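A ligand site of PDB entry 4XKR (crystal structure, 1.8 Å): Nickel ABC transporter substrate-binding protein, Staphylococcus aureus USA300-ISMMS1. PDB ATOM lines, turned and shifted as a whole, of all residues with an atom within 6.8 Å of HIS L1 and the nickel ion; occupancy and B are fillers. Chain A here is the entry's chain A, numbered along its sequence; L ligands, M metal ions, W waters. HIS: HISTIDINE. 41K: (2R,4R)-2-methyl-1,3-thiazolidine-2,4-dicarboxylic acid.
An oxygen (OXT) of HIS L1 sits at hydrogen-bond distance from the side-chain hydroxyl (OH) of Tyr 322 (2.7 Å).
The guanidinium group of Arg 325 lies within salt-bridge range of an oxygen (OXT) of HIS L1 (2.9 Å).
N of HIS L1 lies close to O of Ser 370 (3.1 Å).
NH1 of Arg 234 lies close to O of HIS L1.
A nitrogen (N) of HIS L1 sits close to the side-chain hydroxyl (OH) of Tyr 369, 3.1 Å away.
A nitrogen (N) of HIS L1 sits close to the side-chain carboxylate (OE2) of Glu 355, at 3.8 Å.
An oxygen (OXT) of 41K L2 sits close to the guanidinium group (NH2) of Arg 325, at 3.8 Å.
OAD of 41K L2 is in salt-bridge range of NH2 of Arg 234 (3.8 Å).
N of Gly 372 lies within hydrogen-bond range of OAD of 41K L2, 2.8 Å away.
The side-chain hydroxyl (OH) of Tyr 322 sits at hydrogen-bond distance from the backbone NH (N) of Ser 370, 3.4 Å away.
The side-chain hydroxyl (OG) of Ser 370 is in hydrogen-bond range of the guanidinium group (NH1) of Arg 234, at 3.0 Å.
The side-chain carboxylate (OE1) of Glu 355 lies within salt-bridge range of the side-chain amino group (NZ) of Lys 395 (3.9 Å).
Merely in contact with HIS L1: Leu 17 and Ile 354.
Hydrophobic or aromatic side chains within 4 Å of HIS L1: Leu 17, Tyr 322, Ile 354 and Tyr 369.
Of the 20 residues printed, 8 come within 4 Å of HIS L1.
No residue comes within 4 Å of the nickel ion.
The nickel ion is bound by an oxygen (OAA) of 41K L2 (2.0 Å), a nitrogen (N) of HIS L1 (2.1 Å), an oxygen (O) of HIS L1 (2.1 Å), a nitrogen (ND1) of HIS L1 (2.1 Å), a nitrogen (N) of 41K L2 (2.1 Å) and an oxygen (OXT) of 41K L2 (2.1 Å).
Water W1 lies within hydrogen-bond range of a nitrogen (NE2) of HIS L1 (2.8 Å), the backbone carbonyl oxygen of Leu 17 (2.9 Å) and the backbone carbonyl oxygen of Lys 18 (3.5 Å).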
ATOM      1  N   PRO A  16       5.305  17.759 -29.907  1.00  0.00           N
ATOM      2  CA  PRO A  16       6.079  18.176 -28.744  1.00  0.00           C
ATOM      3  C   PRO A  16       7.175  19.155 -29.170  1.00  0.00           C
ATOM      4  O   PRO A  16       7.346  19.395 -30.386  1.00  0.00           O
ATOM      5  CB  PRO A  16       6.679  16.861 -28.233  1.00  0.00           C
ATOM      6  CG  PRO A  16       6.939  16.092 -29.507  1.00  0.00           C
ATOM      7  CD  PRO A  16       5.834  16.509 -30.498  1.00  0.00           C
ATOM      8  N   LEU A  17       7.915  19.645 -28.180  1.00  0.00           N
ATOM      9  CA  LEU A  17       9.142  20.452 -28.364  1.00  0.00           C
ATOM     10  C   LEU A  17       8.870  21.808 -29.010  1.00  0.00           C
ATOM     11  O   LEU A  17       9.283  22.082 -30.146  1.00  0.00           O
ATOM     12  CB  LEU A  17      10.203  19.666 -29.168  1.00  0.00           C
ATOM     13  CG  LEU A  17      10.515  18.277 -28.582  1.00  0.00           C
ATOM     14  CD1 LEU A  17      11.669  17.576 -29.367  1.00  0.00           C
ATOM     15  CD2 LEU A  17      10.813  18.351 -27.082  1.00  0.00           C
ATOM     16  N   LYS A  18       8.175  22.653 -28.249  1.00  0.00           N
ATOM     17  CA  LYS A  18       7.833  23.999 -28.706  1.00  0.00           C
ATOM     18  C   LYS A  18       9.055  24.748 -29.186  1.00  0.00           C
ATOM     19  O   LYS A  18      10.153  24.619 -28.618  1.00  0.00           O
ATOM     20  CB  LYS A  18       7.151  24.801 -27.586  1.00  0.00           C
ATOM     21  CG  LYS A  18       7.996  24.885 -26.307  1.00  0.00           C
ATOM     22  CD  LYS A  18       7.247  25.598 -25.184  1.00  0.00           C
ATOM     23  CE  LYS A  18       6.044  24.805 -24.736  1.00  0.00           C
ATOM     24  NZ  LYS A  18       5.239  25.563 -23.733  1.00  0.00           N
ATOM     25  N   THR A  19       8.830  25.549 -30.228  1.00  0.00           N
ATOM     26  CA  THR A  19       9.842  26.404 -30.842  1.00  0.00           C
ATOM     27  C   THR A  19       9.733  27.846 -30.342  1.00  0.00           C
ATOM     28  O   THR A  19       8.688  28.252 -29.851  1.00  0.00           O
ATOM     29  CB  THR A  19       9.665  26.432 -32.331  1.00  0.00           C
ATOM     30  OG1 THR A  19       8.291  26.749 -32.611  1.00  0.00           O
ATOM     31  CG2 THR A  19      10.010  25.057 -32.929  1.00  0.00           C
ATOM     32  N   THR A  27      15.060  25.568 -36.720  1.00  0.00           N
ATOM     33  CA  THR A  27      14.277  24.377 -36.384  1.00  0.00           C
ATOM     34  C   THR A  27      13.848  23.638 -37.644  1.00  0.00           C
ATOM     35  O   THR A  27      13.688  24.247 -38.689  1.00  0.00           O
ATOM     36  CB  THR A  27      13.020  24.748 -35.568  1.00  0.00           C
ATOM     37  OG1 THR A  27      12.145  23.609 -35.476  1.00  0.00           O
ATOM     38  CG2 THR A  27      12.294  25.892 -36.231  1.00  0.00           C
ATOM     39  N   ASP A  28      13.687  22.315 -37.531  1.00  0.00           N
ATOM     40  CA  ASP A  28      13.222  21.525 -38.668  1.00  0.00           C
ATOM     41  C   ASP A  28      11.704  21.536 -38.812  1.00  0.00           C
ATOM     42  O   ASP A  28      11.163  20.914 -39.714  1.00  0.00           O
ATOM     43  CB  ASP A  28      13.761  20.103 -38.558  1.00  0.00           C
ATOM     44  CG  ASP A  28      13.028  19.233 -37.533  1.00  0.00           C
ATOM     45  OD1 ASP A  28      12.203  19.740 -36.748  1.00  0.00           O
ATOM     46  OD2 ASP A  28      13.321  18.021 -37.505  1.00  0.00           O
ATOM     47  N   ARG A 234      16.878   7.637 -34.115  1.00  0.00           N
ATOM     48  CA  ARG A 234      16.874   8.490 -32.923  1.00  0.00           C
ATOM     49  C   ARG A 234      17.308   7.667 -31.707  1.00  0.00           C
ATOM     50  O   ARG A 234      16.890   6.516 -31.530  1.00  0.00           O
ATOM     51  CB  ARG A 234      15.493   9.087 -32.686  1.00  0.00           C
ATOM     52  CG  ARG A 234      15.439  10.053 -31.475  1.00  0.00           C
ATOM     53  CD  ARG A 234      14.359  11.096 -31.646  1.00  0.00           C
ATOM     54  NE  ARG A 234      14.721  12.169 -32.580  1.00  0.00           N
ATOM     55  CZ  ARG A 234      15.454  13.237 -32.269  1.00  0.00           C
ATOM     56  NH1 ARG A 234      15.944  13.401 -31.040  1.00  0.00           N
ATOM     57  NH2 ARG A 234      15.698  14.160 -33.212  1.00  0.00           N
ATOM     58  N   TYR A 322      12.576  16.402 -19.583  1.00  0.00           N
ATOM     59  CA  TYR A 322      11.494  17.125 -20.251  1.00  0.00           C
ATOM     60  C   TYR A 322      10.492  16.117 -20.772  1.00  0.00           C
ATOM     61  O   TYR A 322      10.826  14.938 -20.956  1.00  0.00           O
ATOM     62  CB  TYR A 322      12.023  18.019 -21.384  1.00  0.00           C
ATOM     63  CG  TYR A 322      12.871  17.320 -22.440  1.00  0.00           C
ATOM     64  CD1 TYR A 322      14.167  16.883 -22.145  1.00  0.00           C
ATOM     65  CD2 TYR A 322      12.376  17.101 -23.736  1.00  0.00           C
ATOM     66  CE1 TYR A 322      14.952  16.246 -23.107  1.00  0.00           C
ATOM     67  CE2 TYR A 322      13.166  16.477 -24.701  1.00  0.00           C
ATOM     68  CZ  TYR A 322      14.442  16.058 -24.380  1.00  0.00           C
ATOM     69  OH  TYR A 322      15.235  15.435 -25.331  1.00  0.00           O
ATOM     70  N   GLY A 324       8.747  16.076 -23.730  1.00  0.00           N
ATOM     71  CA  GLY A 324       8.548  15.939 -25.171  1.00  0.00           C
ATOM     72  C   GLY A 324       8.724  14.525 -25.720  1.00  0.00           C
ATOM     73  O   GLY A 324       7.885  14.041 -26.486  1.00  0.00           O
ATOM     74  N   ARG A 325       9.815  13.880 -25.333  1.00  0.00           N
ATOM     75  CA  ARG A 325      10.010  12.462 -25.608  1.00  0.00           C
ATOM     76  C   ARG A 325       9.514  11.744 -24.350  1.00  0.00           C
ATOM     77  O   ARG A 325      10.131  11.833 -23.296  1.00  0.00           O
ATOM     78  CB  ARG A 325      11.489  12.128 -25.876  1.00  0.00           C
ATOM     79  CG  ARG A 325      12.231  13.037 -26.833  1.00  0.00           C
ATOM     80  CD  ARG A 325      11.724  12.908 -28.288  1.00  0.00           C
ATOM     81  NE  ARG A 325      12.480  13.803 -29.167  1.00  0.00           N
ATOM     82  CZ  ARG A 325      12.216  13.995 -30.461  1.00  0.00           C
ATOM     83  NH1 ARG A 325      11.221  13.340 -31.041  1.00  0.00           N
ATOM     84  NH2 ARG A 325      12.975  14.832 -31.183  1.00  0.00           N
ATOM     85  N   LEU A 328      11.639   9.640 -21.567  1.00  0.00           N
ATOM     86  CA  LEU A 328      12.816  10.176 -20.903  1.00  0.00           C
ATOM     87  C   LEU A 328      12.609  10.364 -19.401  1.00  0.00           C
ATOM     88  O   LEU A 328      13.485  10.017 -18.611  1.00  0.00           O
ATOM     89  CB  LEU A 328      13.236  11.510 -21.519  1.00  0.00           C
ATOM     90  CG  LEU A 328      13.816  11.431 -22.938  1.00  0.00           C
ATOM     91  CD1 LEU A 328      14.288  12.839 -23.369  1.00  0.00           C
ATOM     92  CD2 LEU A 328      14.952  10.437 -23.028  1.00  0.00           C
ATOM     93  N   ASP A 353      11.001  24.034 -21.513  1.00  0.00           N
ATOM     94  CA  ASP A 353      11.797  24.454 -22.675  1.00  0.00           C
ATOM     95  C   ASP A 353      13.230  23.932 -22.499  1.00  0.00           C
ATOM     96  O   ASP A 353      14.076  24.585 -21.894  1.00  0.00           O
ATOM     97  CB  ASP A 353      11.769  25.991 -22.828  1.00  0.00           C
ATOM     98  CG  ASP A 353      12.777  26.527 -23.850  1.00  0.00           C
ATOM     99  OD1 ASP A 353      13.323  25.757 -24.665  1.00  0.00           O
ATOM    100  OD2 ASP A 353      13.019  27.758 -23.839  1.00  0.00           O
ATOM    101  N   ILE A 354      13.500  22.747 -23.032  1.00  0.00           N
ATOM    102  CA  ILE A 354      14.724  22.070 -22.685  1.00  0.00           C
ATOM    103  C   ILE A 354      15.950  22.814 -23.231  1.00  0.00           C
ATOM    104  O   ILE A 354      16.905  23.018 -22.482  1.00  0.00           O
ATOM    105  CB  ILE A 354      14.692  20.586 -23.151  1.00  0.00           C
ATOM    106  CG1 ILE A 354      16.002  19.872 -22.751  1.00  0.00           C
ATOM    107  CG2 ILE A 354      14.385  20.461 -24.653  1.00  0.00           C
ATOM    108  CD1 ILE A 354      16.208  19.767 -21.243  1.00  0.00           C
ATOM    109  N   GLU A 355      15.937  23.274 -24.480  1.00  0.00           N
ATOM    110  CA  GLU A 355      17.126  23.943 -25.011  1.00  0.00           C
ATOM    111  C   GLU A 355      17.338  25.297 -24.355  1.00  0.00           C
ATOM    112  O   GLU A 355      18.478  25.689 -24.117  1.00  0.00           O
ATOM    113  CB  GLU A 355      17.042  24.109 -26.527  1.00  0.00           C
ATOM    114  CG  GLU A 355      17.020  22.799 -27.289  1.00  0.00           C
ATOM    115  CD  GLU A 355      18.178  21.867 -26.927  1.00  0.00           C
ATOM    116  OE1 GLU A 355      19.132  22.255 -26.213  1.00  0.00           O
ATOM    117  OE2 GLU A 355      18.140  20.721 -27.388  1.00  0.00           O
ATOM    118  N   LEU A 358      19.118  24.346 -21.068  1.00  0.00           N
ATOM    119  CA  LEU A 358      20.477  23.816 -21.091  1.00  0.00           C
ATOM    120  C   LEU A 358      21.524  24.842 -21.522  1.00  0.00           C
ATOM    121  O   LEU A 358      22.725  24.618 -21.335  1.00  0.00           O
ATOM    122  CB  LEU A 358      20.551  22.589 -22.009  1.00  0.00           C
ATOM    123  CG  LEU A 358      19.682  21.388 -21.649  1.00  0.00           C
ATOM    124  CD1 LEU A 358      19.795  20.331 -22.737  1.00  0.00           C
ATOM    125  CD2 LEU A 358      20.105  20.807 -20.287  1.00  0.00           C
ATOM    126  N   TYR A 369      18.233  13.228 -22.693  1.00  0.00           N
ATOM    127  CA  TYR A 369      18.286  13.878 -23.982  1.00  0.00           C
ATOM    128  C   TYR A 369      17.961  12.892 -25.083  1.00  0.00           C
ATOM    129  O   TYR A 369      17.842  11.700 -24.830  1.00  0.00           O
ATOM    130  CB  TYR A 369      19.656  14.524 -24.178  1.00  0.00           C
ATOM    131  CG  TYR A 369      19.641  15.726 -25.101  1.00  0.00           C
ATOM    132  CD1 TYR A 369      19.022  16.927 -24.718  1.00  0.00           C
ATOM    133  CD2 TYR A 369      20.216  15.647 -26.357  1.00  0.00           C
ATOM    134  CE1 TYR A 369      19.026  18.039 -25.595  1.00  0.00           C
ATOM    135  CE2 TYR A 369      20.210  16.755 -27.225  1.00  0.00           C
ATOM    136  CZ  TYR A 369      19.622  17.929 -26.848  1.00  0.00           C
ATOM    137  OH  TYR A 369      19.637  18.977 -27.760  1.00  0.00           O
ATOM    138  N   SER A 370      17.807  13.394 -26.298  1.00  0.00           N
ATOM    139  CA  SER A 370      17.499  12.556 -27.437  1.00  0.00           C
ATOM    140  C   SER A 370      18.121  13.187 -28.664  1.00  0.00           C
ATOM    141  O   SER A 370      17.938  14.385 -28.896  1.00  0.00           O
ATOM    142  CB  SER A 370      15.985  12.413 -27.623  1.00  0.00           C
ATOM    143  OG  SER A 370      15.691  11.537 -28.689  1.00  0.00           O
ATOM    144  N   PHE A 371      18.870  12.398 -29.429  1.00  0.00           N
ATOM    145  CA  PHE A 371      19.579  12.885 -30.610  1.00  0.00           C
ATOM    146  C   PHE A 371      19.064  12.178 -31.864  1.00  0.00           C
ATOM    147  O   PHE A 371      18.901  10.960 -31.846  1.00  0.00           O
ATOM    148  CB  PHE A 371      21.099  12.582 -30.524  1.00  0.00           C
ATOM    149  CG  PHE A 371      21.951  13.630 -29.819  1.00  0.00           C
ATOM    150  CD1 PHE A 371      21.859  14.971 -30.137  1.00  0.00           C
ATOM    151  CD2 PHE A 371      22.922  13.232 -28.911  1.00  0.00           C
ATOM    152  CE1 PHE A 371      22.689  15.905 -29.520  1.00  0.00           C
ATOM    153  CE2 PHE A 371      23.747  14.153 -28.291  1.00  0.00           C
ATOM    154  CZ  PHE A 371      23.633  15.493 -28.612  1.00  0.00           C
ATOM    155  N   GLY A 372      18.877  12.916 -32.964  1.00  0.00           N
ATOM    156  CA  GLY A 372      18.790  12.253 -34.256  1.00  0.00           C
ATOM    157  C   GLY A 372      20.212  12.070 -34.740  1.00  0.00           C
ATOM    158  O   GLY A 372      20.806  13.021 -35.235  1.00  0.00           O
ATOM    159  N   LYS A 395      25.564  20.189 -26.349  1.00  0.00           N
ATOM    160  CA  LYS A 395      25.046  21.003 -25.258  1.00  0.00           C
ATOM    161  C   LYS A 395      25.917  20.915 -23.995  1.00  0.00           C
ATOM    162  O   LYS A 395      25.990  21.892 -23.244  1.00  0.00           O
ATOM    163  CB  LYS A 395      23.588  20.627 -24.913  1.00  0.00           C
ATOM    164  CG  LYS A 395      22.618  20.547 -26.122  1.00  0.00           C
ATOM    165  CD  LYS A 395      22.755  21.747 -27.050  1.00  0.00           C
ATOM    166  CE  LYS A 395      21.657  21.759 -28.122  1.00  0.00           C
ATOM    167  NZ  LYS A 395      21.758  22.986 -28.968  1.00  0.00           N
HETATM  168  N   HIS L   1      17.269  17.384 -29.009  1.00  0.00           N
HETATM  169  CA  HIS L   1      16.199  17.136 -28.036  1.00  0.00           C
HETATM  170  C   HIS L   1      15.118  16.250 -28.634  1.00  0.00           C
HETATM  171  O   HIS L   1      15.040  16.121 -29.859  1.00  0.00           O
HETATM  172  CB  HIS L   1      15.600  18.451 -27.527  1.00  0.00           C
HETATM  173  CG  HIS L   1      14.919  19.282 -28.589  1.00  0.00           C
HETATM  174  ND1 HIS L   1      15.103  19.083 -29.937  1.00  0.00           N
HETATM  175  CD2 HIS L   1      14.063  20.325 -28.468  1.00  0.00           C
HETATM  176  CE1 HIS L   1      14.372  19.975 -30.616  1.00  0.00           C
HETATM  177  NE2 HIS L   1      13.746  20.730 -29.742  1.00  0.00           N
HETATM  178  OXT HIS L   1      14.336  15.640 -27.880  1.00  0.00           O
HETATM  179  OAA 41K L   2      17.286  16.125 -31.694  1.00  0.00           O
HETATM  180  CAE 41K L   2      18.379  16.471 -32.225  1.00  0.00           C
HETATM  181  OAD 41K L   2      19.158  15.709 -32.817  1.00  0.00           O
HETATM  182  CAF 41K L   2      18.709  17.964 -32.235  1.00  0.00           C
HETATM  183  CAB 41K L   2      19.910  18.222 -31.328  1.00  0.00           C
HETATM  184  N   41K L   2      17.619  18.836 -31.745  1.00  0.00           N
HETATM  185  SAK 41K L   2      19.019  18.476 -33.928  1.00  0.00           S
HETATM  186  CB  41K L   2      17.802  19.777 -33.949  1.00  0.00           C
HETATM  187  CA  41K L   2      16.786  19.341 -32.852  1.00  0.00           C
HETATM  188  C   41K L   2      15.680  18.431 -33.419  1.00  0.00           C
HETATM  189  O   41K L   2      15.316  18.711 -34.590  1.00  0.00           O
HETATM  190  OXT 41K L   2      15.210  17.544 -32.654  1.00  0.00           O
HETATM  191 NI    NI M   1      16.228  17.545 -30.783  1.00  0.00          NI
HETATM  192  O   HOH W   1      12.038  22.709 -30.792  1.00  0.00           O
